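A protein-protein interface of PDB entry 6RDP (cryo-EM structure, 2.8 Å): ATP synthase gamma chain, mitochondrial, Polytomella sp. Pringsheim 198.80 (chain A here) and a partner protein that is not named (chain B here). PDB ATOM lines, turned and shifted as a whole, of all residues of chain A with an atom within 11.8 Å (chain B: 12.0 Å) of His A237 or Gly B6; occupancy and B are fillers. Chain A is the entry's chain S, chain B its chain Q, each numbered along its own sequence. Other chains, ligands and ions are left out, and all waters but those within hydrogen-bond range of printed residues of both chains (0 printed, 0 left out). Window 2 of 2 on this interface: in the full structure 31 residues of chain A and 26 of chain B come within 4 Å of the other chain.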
ATOM      1  N   PRO A 213      19.400   4.143 -17.341  1.00  0.00           N
ATOM      2  CA  PRO A 213      18.741   3.503 -18.501  1.00  0.00           C
ATOM      3  C   PRO A 213      19.277   3.798 -19.895  1.00  0.00           C
ATOM      4  O   PRO A 213      19.632   2.873 -20.625  1.00  0.00           O
ATOM      5  CB  PRO A 213      17.299   4.013 -18.385  1.00  0.00           C
ATOM      6  CG  PRO A 213      17.365   5.200 -17.513  1.00  0.00           C
ATOM      7  CD  PRO A 213      18.399   4.855 -16.526  1.00  0.00           C
ATOM      8  N   TYR A 231      14.376  -6.215 -29.768  1.00  0.00           N
ATOM      9  CA  TYR A 231      13.202  -6.504 -28.960  1.00  0.00           C
ATOM     10  C   TYR A 231      12.079  -5.527 -29.259  1.00  0.00           C
ATOM     11  O   TYR A 231      12.309  -4.326 -29.411  1.00  0.00           O
ATOM     12  CB  TYR A 231      13.542  -6.436 -27.471  1.00  0.00           C
ATOM     13  CG  TYR A 231      14.782  -7.196 -27.067  1.00  0.00           C
ATOM     14  CD1 TYR A 231      14.730  -8.550 -26.792  1.00  0.00           C
ATOM     15  CD2 TYR A 231      16.003  -6.551 -26.948  1.00  0.00           C
ATOM     16  CE1 TYR A 231      15.862  -9.248 -26.430  1.00  0.00           C
ATOM     17  CE2 TYR A 231      17.137  -7.238 -26.586  1.00  0.00           C
ATOM     18  CZ  TYR A 231      17.059  -8.584 -26.329  1.00  0.00           C
ATOM     19  OH  TYR A 231      18.190  -9.262 -25.963  1.00  0.00           O
ATOM     20  N   ASP A 232      10.859  -6.047 -29.322  1.00  0.00           N
ATOM     21  CA  ASP A 232       9.682  -5.199 -29.447  1.00  0.00           C
ATOM     22  C   ASP A 232       9.262  -4.714 -28.072  1.00  0.00           C
ATOM     23  O   ASP A 232       8.798  -5.505 -27.248  1.00  0.00           O
ATOM     24  CB  ASP A 232       8.528  -5.946 -30.107  1.00  0.00           C
ATOM     25  CG  ASP A 232       8.872  -6.446 -31.479  1.00  0.00           C
ATOM     26  OD1 ASP A 232       8.286  -7.466 -31.893  1.00  0.00           O
ATOM     27  OD2 ASP A 232       9.730  -5.824 -32.140  1.00  0.00           O
ATOM     28  N   ILE A 233       9.404  -3.416 -27.833  1.00  0.00           N
ATOM     29  CA  ILE A 233       8.987  -2.839 -26.564  1.00  0.00           C
ATOM     30  C   ILE A 233       7.468  -2.846 -26.489  1.00  0.00           C
ATOM     31  O   ILE A 233       6.790  -2.182 -27.278  1.00  0.00           O
ATOM     32  CB  ILE A 233       9.535  -1.421 -26.404  1.00  0.00           C
ATOM     33  CG1 ILE A 233      11.054  -1.429 -26.544  1.00  0.00           C
ATOM     34  CG2 ILE A 233       9.086  -0.847 -25.091  1.00  0.00           C
ATOM     35  CD1 ILE A 233      11.740  -2.296 -25.539  1.00  0.00           C
ATOM     36  N   GLU A 234       6.932  -3.579 -25.528  1.00  0.00           N
ATOM     37  CA  GLU A 234       5.498  -3.726 -25.357  1.00  0.00           C
ATOM     38  C   GLU A 234       5.073  -2.983 -24.098  1.00  0.00           C
ATOM     39  O   GLU A 234       4.280  -3.459 -23.299  1.00  0.00           O
ATOM     40  CB  GLU A 234       5.130  -5.209 -25.329  1.00  0.00           C
ATOM     41  CG  GLU A 234       3.679  -5.597 -25.659  1.00  0.00           C
ATOM     42  CD  GLU A 234       2.808  -5.811 -24.437  1.00  0.00           C
ATOM     43  OE1 GLU A 234       3.339  -6.165 -23.377  1.00  0.00           O
ATOM     44  OE2 GLU A 234       1.579  -5.634 -24.535  1.00  0.00           O
ATOM     45  N   ALA A 235       5.627  -1.801 -23.890  1.00  0.00           N
ATOM     46  CA  ALA A 235       5.307  -1.004 -22.721  1.00  0.00           C
ATOM     47  C   ALA A 235       4.052  -0.182 -22.978  1.00  0.00           C
ATOM     48  O   ALA A 235       3.440  -0.248 -24.045  1.00  0.00           O
ATOM     49  CB  ALA A 235       6.481  -0.101 -22.350  1.00  0.00           C
ATOM     50  N   SER A 236       3.651   0.588 -21.970  1.00  0.00           N
ATOM     51  CA  SER A 236       2.619   1.592 -22.186  1.00  0.00           C
ATOM     52  C   SER A 236       3.203   2.822 -22.863  1.00  0.00           C
ATOM     53  O   SER A 236       2.670   3.308 -23.865  1.00  0.00           O
ATOM     54  CB  SER A 236       1.966   1.974 -20.861  1.00  0.00           C
ATOM     55  OG  SER A 236       2.781   2.886 -20.153  1.00  0.00           O
ATOM     56  N   HIS A 237       4.297   3.344 -22.318  1.00  0.00           N
ATOM     57  CA  HIS A 237       5.005   4.500 -22.824  1.00  0.00           C
ATOM     58  C   HIS A 237       6.280   4.059 -23.541  1.00  0.00           C
ATOM     59  O   HIS A 237       6.443   2.879 -23.866  1.00  0.00           O
ATOM     60  CB  HIS A 237       5.249   5.470 -21.679  1.00  0.00           C
ATOM     61  CG  HIS A 237       3.997   6.111 -21.173  1.00  0.00           C
ATOM     62  ND1 HIS A 237       3.026   5.410 -20.492  1.00  0.00           N
ATOM     63  CD2 HIS A 237       3.546   7.383 -21.266  1.00  0.00           C
ATOM     64  CE1 HIS A 237       2.036   6.224 -20.178  1.00  0.00           C
ATOM     65  NE2 HIS A 237       2.327   7.428 -20.633  1.00  0.00           N
ATOM     66  N   GLU A 238       7.162   5.014 -23.819  1.00  0.00           N
ATOM     67  CA  GLU A 238       8.289   4.802 -24.715  1.00  0.00           C
ATOM     68  C   GLU A 238       9.353   3.910 -24.079  1.00  0.00           C
ATOM     69  O   GLU A 238       9.287   3.549 -22.902  1.00  0.00           O
ATOM     70  CB  GLU A 238       8.893   6.143 -25.114  1.00  0.00           C
ATOM     71  CG  GLU A 238       8.143   6.856 -26.218  1.00  0.00           C
ATOM     72  CD  GLU A 238       8.469   6.298 -27.583  1.00  0.00           C
ATOM     73  OE1 GLU A 238       7.530   6.017 -28.357  1.00  0.00           O
ATOM     74  OE2 GLU A 238       9.668   6.134 -27.880  1.00  0.00           O
ATOM     75  N   ARG A 239      10.362   3.572 -24.888  1.00  0.00           N
ATOM     76  CA  ARG A 239      11.464   2.718 -24.449  1.00  0.00           C
ATOM     77  C   ARG A 239      12.304   3.378 -23.365  1.00  0.00           C
ATOM     78  O   ARG A 239      12.809   2.693 -22.467  1.00  0.00           O
ATOM     79  CB  ARG A 239      12.340   2.353 -25.646  1.00  0.00           C
ATOM     80  CG  ARG A 239      13.473   1.407 -25.319  1.00  0.00           C
ATOM     81  CD  ARG A 239      14.092   0.781 -26.531  1.00  0.00           C
ATOM     82  NE  ARG A 239      14.791   1.758 -27.348  1.00  0.00           N
ATOM     83  CZ  ARG A 239      15.629   1.432 -28.321  1.00  0.00           C
ATOM     84  NH1 ARG A 239      15.868   0.156 -28.579  1.00  0.00           N
ATOM     85  NH2 ARG A 239      16.229   2.377 -29.030  1.00  0.00           N
ATOM     86  N   SER A 240      12.417   4.703 -23.398  1.00  0.00           N
ATOM     87  CA  SER A 240      13.157   5.453 -22.393  1.00  0.00           C
ATOM     88  C   SER A 240      12.553   5.355 -21.001  1.00  0.00           C
ATOM     89  O   SER A 240      13.234   5.674 -20.025  1.00  0.00           O
ATOM     90  CB  SER A 240      13.225   6.922 -22.807  1.00  0.00           C
ATOM     91  OG  SER A 240      13.850   7.701 -21.806  1.00  0.00           O
ATOM     92  N   ASP A 241      11.299   4.931 -20.887  1.00  0.00           N
ATOM     93  CA  ASP A 241      10.656   4.712 -19.609  1.00  0.00           C
ATOM     94  C   ASP A 241      10.572   3.239 -19.238  1.00  0.00           C
ATOM     95  O   ASP A 241      10.589   2.915 -18.044  1.00  0.00           O
ATOM     96  CB  ASP A 241       9.263   5.333 -19.634  1.00  0.00           C
ATOM     97  CG  ASP A 241       9.308   6.801 -19.988  1.00  0.00           C
ATOM     98  OD1 ASP A 241      10.415   7.373 -20.001  1.00  0.00           O
ATOM     99  OD2 ASP A 241       8.253   7.379 -20.309  1.00  0.00           O
ATOM    100  N   VAL A 242      10.529   2.340 -20.217  1.00  0.00           N
ATOM    101  CA  VAL A 242      10.604   0.929 -19.882  1.00  0.00           C
ATOM    102  C   VAL A 242      12.014   0.567 -19.425  1.00  0.00           C
ATOM    103  O   VAL A 242      12.167  -0.264 -18.532  1.00  0.00           O
ATOM    104  CB  VAL A 242      10.115   0.032 -21.040  1.00  0.00           C
ATOM    105  CG1 VAL A 242      11.152  -0.181 -22.107  1.00  0.00           C
ATOM    106  CG2 VAL A 242       9.663  -1.293 -20.526  1.00  0.00           C
ATOM    107  N   LEU A 243      13.052   1.249 -19.922  1.00  0.00           N
ATOM    108  CA  LEU A 243      14.381   1.016 -19.367  1.00  0.00           C
ATOM    109  C   LEU A 243      14.556   1.715 -18.035  1.00  0.00           C
ATOM    110  O   LEU A 243      15.312   1.236 -17.190  1.00  0.00           O
ATOM    111  CB  LEU A 243      15.469   1.453 -20.338  1.00  0.00           C
ATOM    112  CG  LEU A 243      16.008   0.382 -21.277  1.00  0.00           C
ATOM    113  CD1 LEU A 243      15.008  -0.048 -22.317  1.00  0.00           C
ATOM    114  CD2 LEU A 243      17.260   0.897 -21.934  1.00  0.00           C
ATOM    115  N   ARG A 244      13.844   2.820 -17.833  1.00  0.00           N
ATOM    116  CA  ARG A 244      13.855   3.497 -16.545  1.00  0.00           C
ATOM    117  C   ARG A 244      13.261   2.616 -15.460  1.00  0.00           C
ATOM    118  O   ARG A 244      13.816   2.517 -14.365  1.00  0.00           O
ATOM    119  CB  ARG A 244      13.093   4.816 -16.654  1.00  0.00           C
ATOM    120  CG  ARG A 244      12.679   5.444 -15.350  1.00  0.00           C
ATOM    121  CD  ARG A 244      13.861   5.972 -14.574  1.00  0.00           C
ATOM    122  NE  ARG A 244      14.755   6.771 -15.399  1.00  0.00           N
ATOM    123  CZ  ARG A 244      15.807   7.431 -14.926  1.00  0.00           C
ATOM    124  NH1 ARG A 244      16.580   8.133 -15.746  1.00  0.00           N
ATOM    125  NH2 ARG A 244      16.086   7.392 -13.629  1.00  0.00           N
ATOM    126  N   ASP A 245      12.152   1.941 -15.754  1.00  0.00           N
ATOM    127  CA  ASP A 245      11.592   0.992 -14.798  1.00  0.00           C
ATOM    128  C   ASP A 245      12.436  -0.272 -14.705  1.00  0.00           C
ATOM    129  O   ASP A 245      12.591  -0.851 -13.622  1.00  0.00           O
ATOM    130  CB  ASP A 245      10.162   0.639 -15.194  1.00  0.00           C
ATOM    131  CG  ASP A 245       9.258   1.854 -15.274  1.00  0.00           C
ATOM    132  OD1 ASP A 245       9.562   2.870 -14.617  1.00  0.00           O
ATOM    133  OD2 ASP A 245       8.238   1.790 -15.992  1.00  0.00           O
ATOM    134  N   LEU A 246      13.023  -0.684 -15.824  1.00  0.00           N
ATOM    135  CA  LEU A 246      13.715  -1.958 -15.891  1.00  0.00           C
ATOM    136  C   LEU A 246      15.045  -1.917 -15.154  1.00  0.00           C
ATOM    137  O   LEU A 246      15.445  -2.915 -14.552  1.00  0.00           O
ATOM    138  CB  LEU A 246      13.884  -2.328 -17.363  1.00  0.00           C
ATOM    139  CG  LEU A 246      14.214  -3.740 -17.797  1.00  0.00           C
ATOM    140  CD1 LEU A 246      13.272  -4.664 -17.137  1.00  0.00           C
ATOM    141  CD2 LEU A 246      14.045  -3.849 -19.285  1.00  0.00           C
ATOM    142  N   GLU A 248      15.624   0.121 -12.468  1.00  0.00           N
ATOM    143  CA  GLU A 248      15.310   0.116 -11.044  1.00  0.00           C
ATOM    144  C   GLU A 248      14.952  -1.283 -10.573  1.00  0.00           C
ATOM    145  O   GLU A 248      15.314  -1.682  -9.461  1.00  0.00           O
ATOM    146  CB  GLU A 248      14.184   1.091 -10.727  1.00  0.00           C
ATOM    147  CG  GLU A 248      14.456   2.486 -11.206  1.00  0.00           C
ATOM    148  CD  GLU A 248      13.238   3.371 -11.141  1.00  0.00           C
ATOM    149  OE1 GLU A 248      12.133   2.853 -10.882  1.00  0.00           O
ATOM    150  OE2 GLU A 248      13.385   4.590 -11.357  1.00  0.00           O
ATOM    151  N   ALA B   3       4.967  16.496 -13.459  1.00  0.00           N
ATOM    152  CA  ALA B   3       6.275  16.957 -13.926  1.00  0.00           C
ATOM    153  C   ALA B   3       7.109  15.951 -14.775  1.00  0.00           C
ATOM    154  O   ALA B   3       7.643  16.369 -15.802  1.00  0.00           O
ATOM    155  CB  ALA B   3       7.105  17.469 -12.727  1.00  0.00           C
ATOM    156  N   PRO B   4       7.243  14.666 -14.408  1.00  0.00           N
ATOM    157  CA  PRO B   4       7.943  13.745 -15.308  1.00  0.00           C
ATOM    158  C   PRO B   4       7.008  13.250 -16.401  1.00  0.00           C
ATOM    159  O   PRO B   4       5.807  13.507 -16.397  1.00  0.00           O
ATOM    160  CB  PRO B   4       8.381  12.592 -14.393  1.00  0.00           C
ATOM    161  CG  PRO B   4       8.042  13.022 -13.008  1.00  0.00           C
ATOM    162  CD  PRO B   4       6.890  13.935 -13.175  1.00  0.00           C
ATOM    163  N   SER B   5       7.589  12.517 -17.348  1.00  0.00           N
ATOM    164  CA  SER B   5       6.857  11.988 -18.494  1.00  0.00           C
ATOM    165  C   SER B   5       7.032  10.477 -18.523  1.00  0.00           C
ATOM    166  O   SER B   5       8.099   9.978 -18.892  1.00  0.00           O
ATOM    167  CB  SER B   5       7.344  12.621 -19.796  1.00  0.00           C
ATOM    168  OG  SER B   5       8.730  12.397 -19.990  1.00  0.00           O
ATOM    169  N   GLY B   6       5.985   9.754 -18.143  1.00  0.00           N
ATOM    170  CA  GLY B   6       6.028   8.316 -18.147  1.00  0.00           C
ATOM    171  C   GLY B   6       4.690   7.690 -17.834  1.00  0.00           C
ATOM    172  O   GLY B   6       3.633   8.269 -18.091  1.00  0.00           O
ATOM    173  N   PRO B   7       4.712   6.480 -17.272  1.00  0.00           N
ATOM    174  CA  PRO B   7       3.465   5.848 -16.824  1.00  0.00           C
ATOM    175  C   PRO B   7       2.834   6.543 -15.629  1.00  0.00           C
ATOM    176  O   PRO B   7       3.369   7.526 -15.113  1.00  0.00           O
ATOM    177  CB  PRO B   7       3.905   4.425 -16.469  1.00  0.00           C
ATOM    178  CG  PRO B   7       5.150   4.208 -17.254  1.00  0.00           C
ATOM    179  CD  PRO B   7       5.836   5.529 -17.279  1.00  0.00           C
ATOM    180  N   PHE B   8       1.696   6.016 -15.174  1.00  0.00           N
ATOM    181  CA  PHE B   8       0.898   6.706 -14.167  1.00  0.00           C
ATOM    182  C   PHE B   8       1.565   6.712 -12.803  1.00  0.00           C
ATOM    183  O   PHE B   8       1.275   7.586 -11.982  1.00  0.00           O
ATOM    184  CB  PHE B   8      -0.493   6.085 -14.075  1.00  0.00           C
ATOM    185  CG  PHE B   8      -0.521   4.709 -13.477  1.00  0.00           C
ATOM    186  CD1 PHE B   8      -0.922   4.519 -12.168  1.00  0.00           C
ATOM    187  CD2 PHE B   8      -0.197   3.599 -14.240  1.00  0.00           C
ATOM    188  CE1 PHE B   8      -0.965   3.256 -11.620  1.00  0.00           C
ATOM    189  CE2 PHE B   8      -0.237   2.333 -13.698  1.00  0.00           C
ATOM    190  CZ  PHE B   8      -0.624   2.163 -12.388  1.00  0.00           C
ATOM    191  N   TYR B   9       2.447   5.753 -12.536  1.00  0.00           N
ATOM    192  CA  TYR B   9       3.237   5.822 -11.315  1.00  0.00           C
ATOM    193  C   TYR B   9       4.396   6.797 -11.462  1.00  0.00           C
ATOM    194  O   TYR B   9       4.742   7.497 -10.508  1.00  0.00           O
ATOM    195  CB  TYR B   9       3.745   4.429 -10.930  1.00  0.00           C
ATOM    196  CG  TYR B   9       4.362   3.629 -12.058  1.00  0.00           C
ATOM    197  CD1 TYR B   9       3.608   2.718 -12.778  1.00  0.00           C
ATOM    198  CD2 TYR B   9       5.704   3.762 -12.376  1.00  0.00           C
ATOM    199  CE1 TYR B   9       4.168   1.985 -13.794  1.00  0.00           C
ATOM    200  CE2 TYR B   9       6.271   3.038 -13.394  1.00  0.00           C
ATOM    201  CZ  TYR B   9       5.502   2.152 -14.099  1.00  0.00           C
ATOM    202  OH  TYR B   9       6.076   1.424 -15.113  1.00  0.00           O
ATOM    203  N   ARG B  10       4.979   6.883 -12.655  1.00  0.00           N
ATOM    204  CA  ARG B  10       6.191   7.664 -12.854  1.00  0.00           C
ATOM    205  C   ARG B  10       5.917   9.162 -12.864  1.00  0.00           C
ATOM    206  O   ARG B  10       6.743   9.942 -12.375  1.00  0.00           O
ATOM    207  CB  ARG B  10       6.865   7.239 -14.156  1.00  0.00           C
ATOM    208  CG  ARG B  10       8.198   7.888 -14.405  1.00  0.00           C
ATOM    209  CD  ARG B  10       9.165   7.515 -13.312  1.00  0.00           C
ATOM    210  NE  ARG B  10       9.331   6.073 -13.226  1.00  0.00           N
ATOM    211  CZ  ARG B  10      10.402   5.484 -12.716  1.00  0.00           C
ATOM    212  NH1 ARG B  10      11.393   6.225 -12.246  1.00  0.00           N
ATOM    213  NH2 ARG B  10      10.486   4.166 -12.684  1.00  0.00           N
ATOM    214  N   VAL B  11       4.765   9.579 -13.395  1.00  0.00           N
ATOM    215  CA  VAL B  11       4.428  10.997 -13.419  1.00  0.00           C
ATOM    216  C   VAL B  11       4.053  11.504 -12.035  1.00  0.00           C
ATOM    217  O   VAL B  11       4.148  12.707 -11.773  1.00  0.00           O
ATOM    218  CB  VAL B  11       3.291  11.264 -14.423  1.00  0.00           C
ATOM    219  CG1 VAL B  11       3.760  10.992 -15.836  1.00  0.00           C
ATOM    220  CG2 VAL B  11       2.071  10.418 -14.097  1.00  0.00           C
ATOM    221  N   ALA B  12       3.654  10.614 -11.130  1.00  0.00           N
ATOM    222  CA  ALA B  12       3.259  10.986  -9.781  1.00  0.00           C
ATOM    223  C   ALA B  12       4.435  11.067  -8.819  1.00  0.00           C
ATOM    224  O   ALA B  12       4.218  11.128  -7.605  1.00  0.00           O
ATOM    225  CB  ALA B  12       2.222   9.997  -9.249  1.00  0.00           C
ATOM    226  N   GLY B  13       5.670  11.062  -9.329  1.00  0.00           N
ATOM    227  CA  GLY B  13       6.858  11.067  -8.500  1.00  0.00           C
ATOM    228  C   GLY B  13       7.288   9.715  -7.973  1.00  0.00           C
ATOM    229  O   GLY B  13       8.408   9.596  -7.461  1.00  0.00           O
ATOM    230  N   MET B  14       6.443   8.695  -8.084  1.00  0.00           N
ATOM    231  CA  MET B  14       6.748   7.378  -7.547  1.00  0.00           C
ATOM    232  C   MET B  14       7.750   6.655  -8.437  1.00  0.00           C
ATOM    233  O   MET B  14       7.743   6.811  -9.660  1.00  0.00           O
ATOM    234  CB  MET B  14       5.461   6.564  -7.433  1.00  0.00           C
ATOM    235  CG  MET B  14       5.568   5.297  -6.627  1.00  0.00           C
ATOM    236  SD  MET B  14       4.093   4.287  -6.791  1.00  0.00           S
ATOM    237  CE  MET B  14       2.826   5.475  -6.401  1.00  0.00           C
ATOM    238  N   SER B  15       8.626   5.870  -7.820  1.00  0.00           N
ATOM    239  CA  SER B  15       9.499   4.987  -8.574  1.00  0.00           C
ATOM    240  C   SER B  15       8.713   3.771  -9.055  1.00  0.00           C
ATOM    241  O   SER B  15       7.565   3.545  -8.663  1.00  0.00           O
ATOM    242  CB  SER B  15      10.688   4.558  -7.723  1.00  0.00           C
ATOM    243  OG  SER B  15      10.267   3.722  -6.662  1.00  0.00           O
ATOM    244  N   TYR B  16       9.337   2.969  -9.915  1.00  0.00           N
ATOM    245  CA  TYR B  16       8.672   1.762 -10.382  1.00  0.00           C
ATOM    246  C   TYR B  16       8.648   0.687  -9.312  1.00  0.00           C
ATOM    247  O   TYR B  16       7.664  -0.052  -9.204  1.00  0.00           O
ATOM    248  CB  TYR B  16       9.360   1.220 -11.626  1.00  0.00           C
ATOM    249  CG  TYR B  16       8.883  -0.146 -12.015  1.00  0.00           C
ATOM    250  CD1 TYR B  16       7.615  -0.328 -12.529  1.00  0.00           C
ATOM    251  CD2 TYR B  16       9.692  -1.257 -11.858  1.00  0.00           C
ATOM    252  CE1 TYR B  16       7.168  -1.570 -12.881  1.00  0.00           C
ATOM    253  CE2 TYR B  16       9.249  -2.502 -12.198  1.00  0.00           C
ATOM    254  CZ  TYR B  16       7.988  -2.652 -12.715  1.00  0.00           C
ATOM    255  OH  TYR B  16       7.541  -3.896 -13.068  1.00  0.00           O
ATOM    256  N   TYR B  19       5.793   1.005  -6.905  1.00  0.00           N
ATOM    257  CA  TYR B  19       4.517   0.636  -7.505  1.00  0.00           C
ATOM    258  C   TYR B  19       4.386  -0.873  -7.626  1.00  0.00           C
ATOM    259  O   TYR B  19       3.332  -1.447  -7.319  1.00  0.00           O
ATOM    260  CB  TYR B  19       4.381   1.303  -8.873  1.00  0.00           C
ATOM    261  CG  TYR B  19       3.537   0.539  -9.861  1.00  0.00           C
ATOM    262  CD1 TYR B  19       4.127  -0.179 -10.896  1.00  0.00           C
ATOM    263  CD2 TYR B  19       2.153   0.550  -9.775  1.00  0.00           C
ATOM    264  CE1 TYR B  19       3.366  -0.875 -11.800  1.00  0.00           C
ATOM    265  CE2 TYR B  19       1.385  -0.143 -10.681  1.00  0.00           C
ATOM    266  CZ  TYR B  19       1.997  -0.856 -11.689  1.00  0.00           C
ATOM    267  OH  TYR B  19       1.240  -1.554 -12.598  1.00  0.00           O
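NE2 of His A237 sits at hydrogen-bond distance from O of Gly B6 (3.0 Å). NH2 of Arg B10 is in salt-bridge range of OD1 of Asp A245, at 2.5 Å. OE2 of Glu A248 lies within salt-bridge range of NH1 of Arg B10, at 2.7 Å. The side-chain carboxylate (OE1) of Glu A248 lies within hydrogen-bond range of the backbone NH (N) of Tyr B16 (3.0 Å). The backbone carbonyl oxygen (O) of Ser B5 sits close to the side-chain carboxylate (OD2) of Asp A241. OH of Tyr B9 sits close to OD2 of Asp A245 (2.4 Å).
O of Tyr B9 lies within hydrogen-bond range of N of Met B14 (3.2 Å). OG of Ser A236 is in hydrogen-bond range of ND1 of His A237 (2.6 Å).
Among the printed residues, pairs that only touch across the chains: Asp A241 with Gly B6, Arg A244 with Arg B10, Asp A245 with Tyr B16, His A237 with Pro B7, Glu A248 with Ser B15 and Ser A236 with Pro B7.
Glu A234 touches none of the printed residues of chain B. His A237 touches two residues of chain B. Glu A238 touches none of the printed residues of chain B. Arg A239 touches none of the printed residues of chain B. Of the printed residues of chain B, Arg A244 touches Arg B10 (3.4 Å). Pro B4 touches none of the printed residues of chain A. Ser B5 touches one residue of chain A. Of chain A, only His A237 (3.0 Å) and Asp A241 (3.2 Å) come within 4 Å of Gly B6. Of chain A, only Ser A236 (3.97 Å) and His A237 (3.7 Å) come within 4 Å of Pro B7. Of chain A, only Asp A245 comes within 4 Å of Tyr B9. Printed residues of chain A within 4 Å of Arg B10: Arg A244, Asp A245 and Glu A248. No residue of chain A comes within 4 Å of Val B11.
Hydrophobic or aromatic side chains of chain B within 4 Å of the printed part of chain A: Pro B7, Tyr B9 and Tyr B16. Printed residues of chain A that touch a printed residue of chain B: Ser A236, His A237, Asp A241, Arg A244, Asp A245 and Glu A248. Hydrophobic or aromatic side chains of chain A that line the printed part of chain B: His A237. Among the printed residues, Asp or Glu carboxylates within 4 Å of a Lys or Arg side-chain nitrogen of the other chain: Asp A245 with Arg B10 and Glu A248 with Arg B10.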
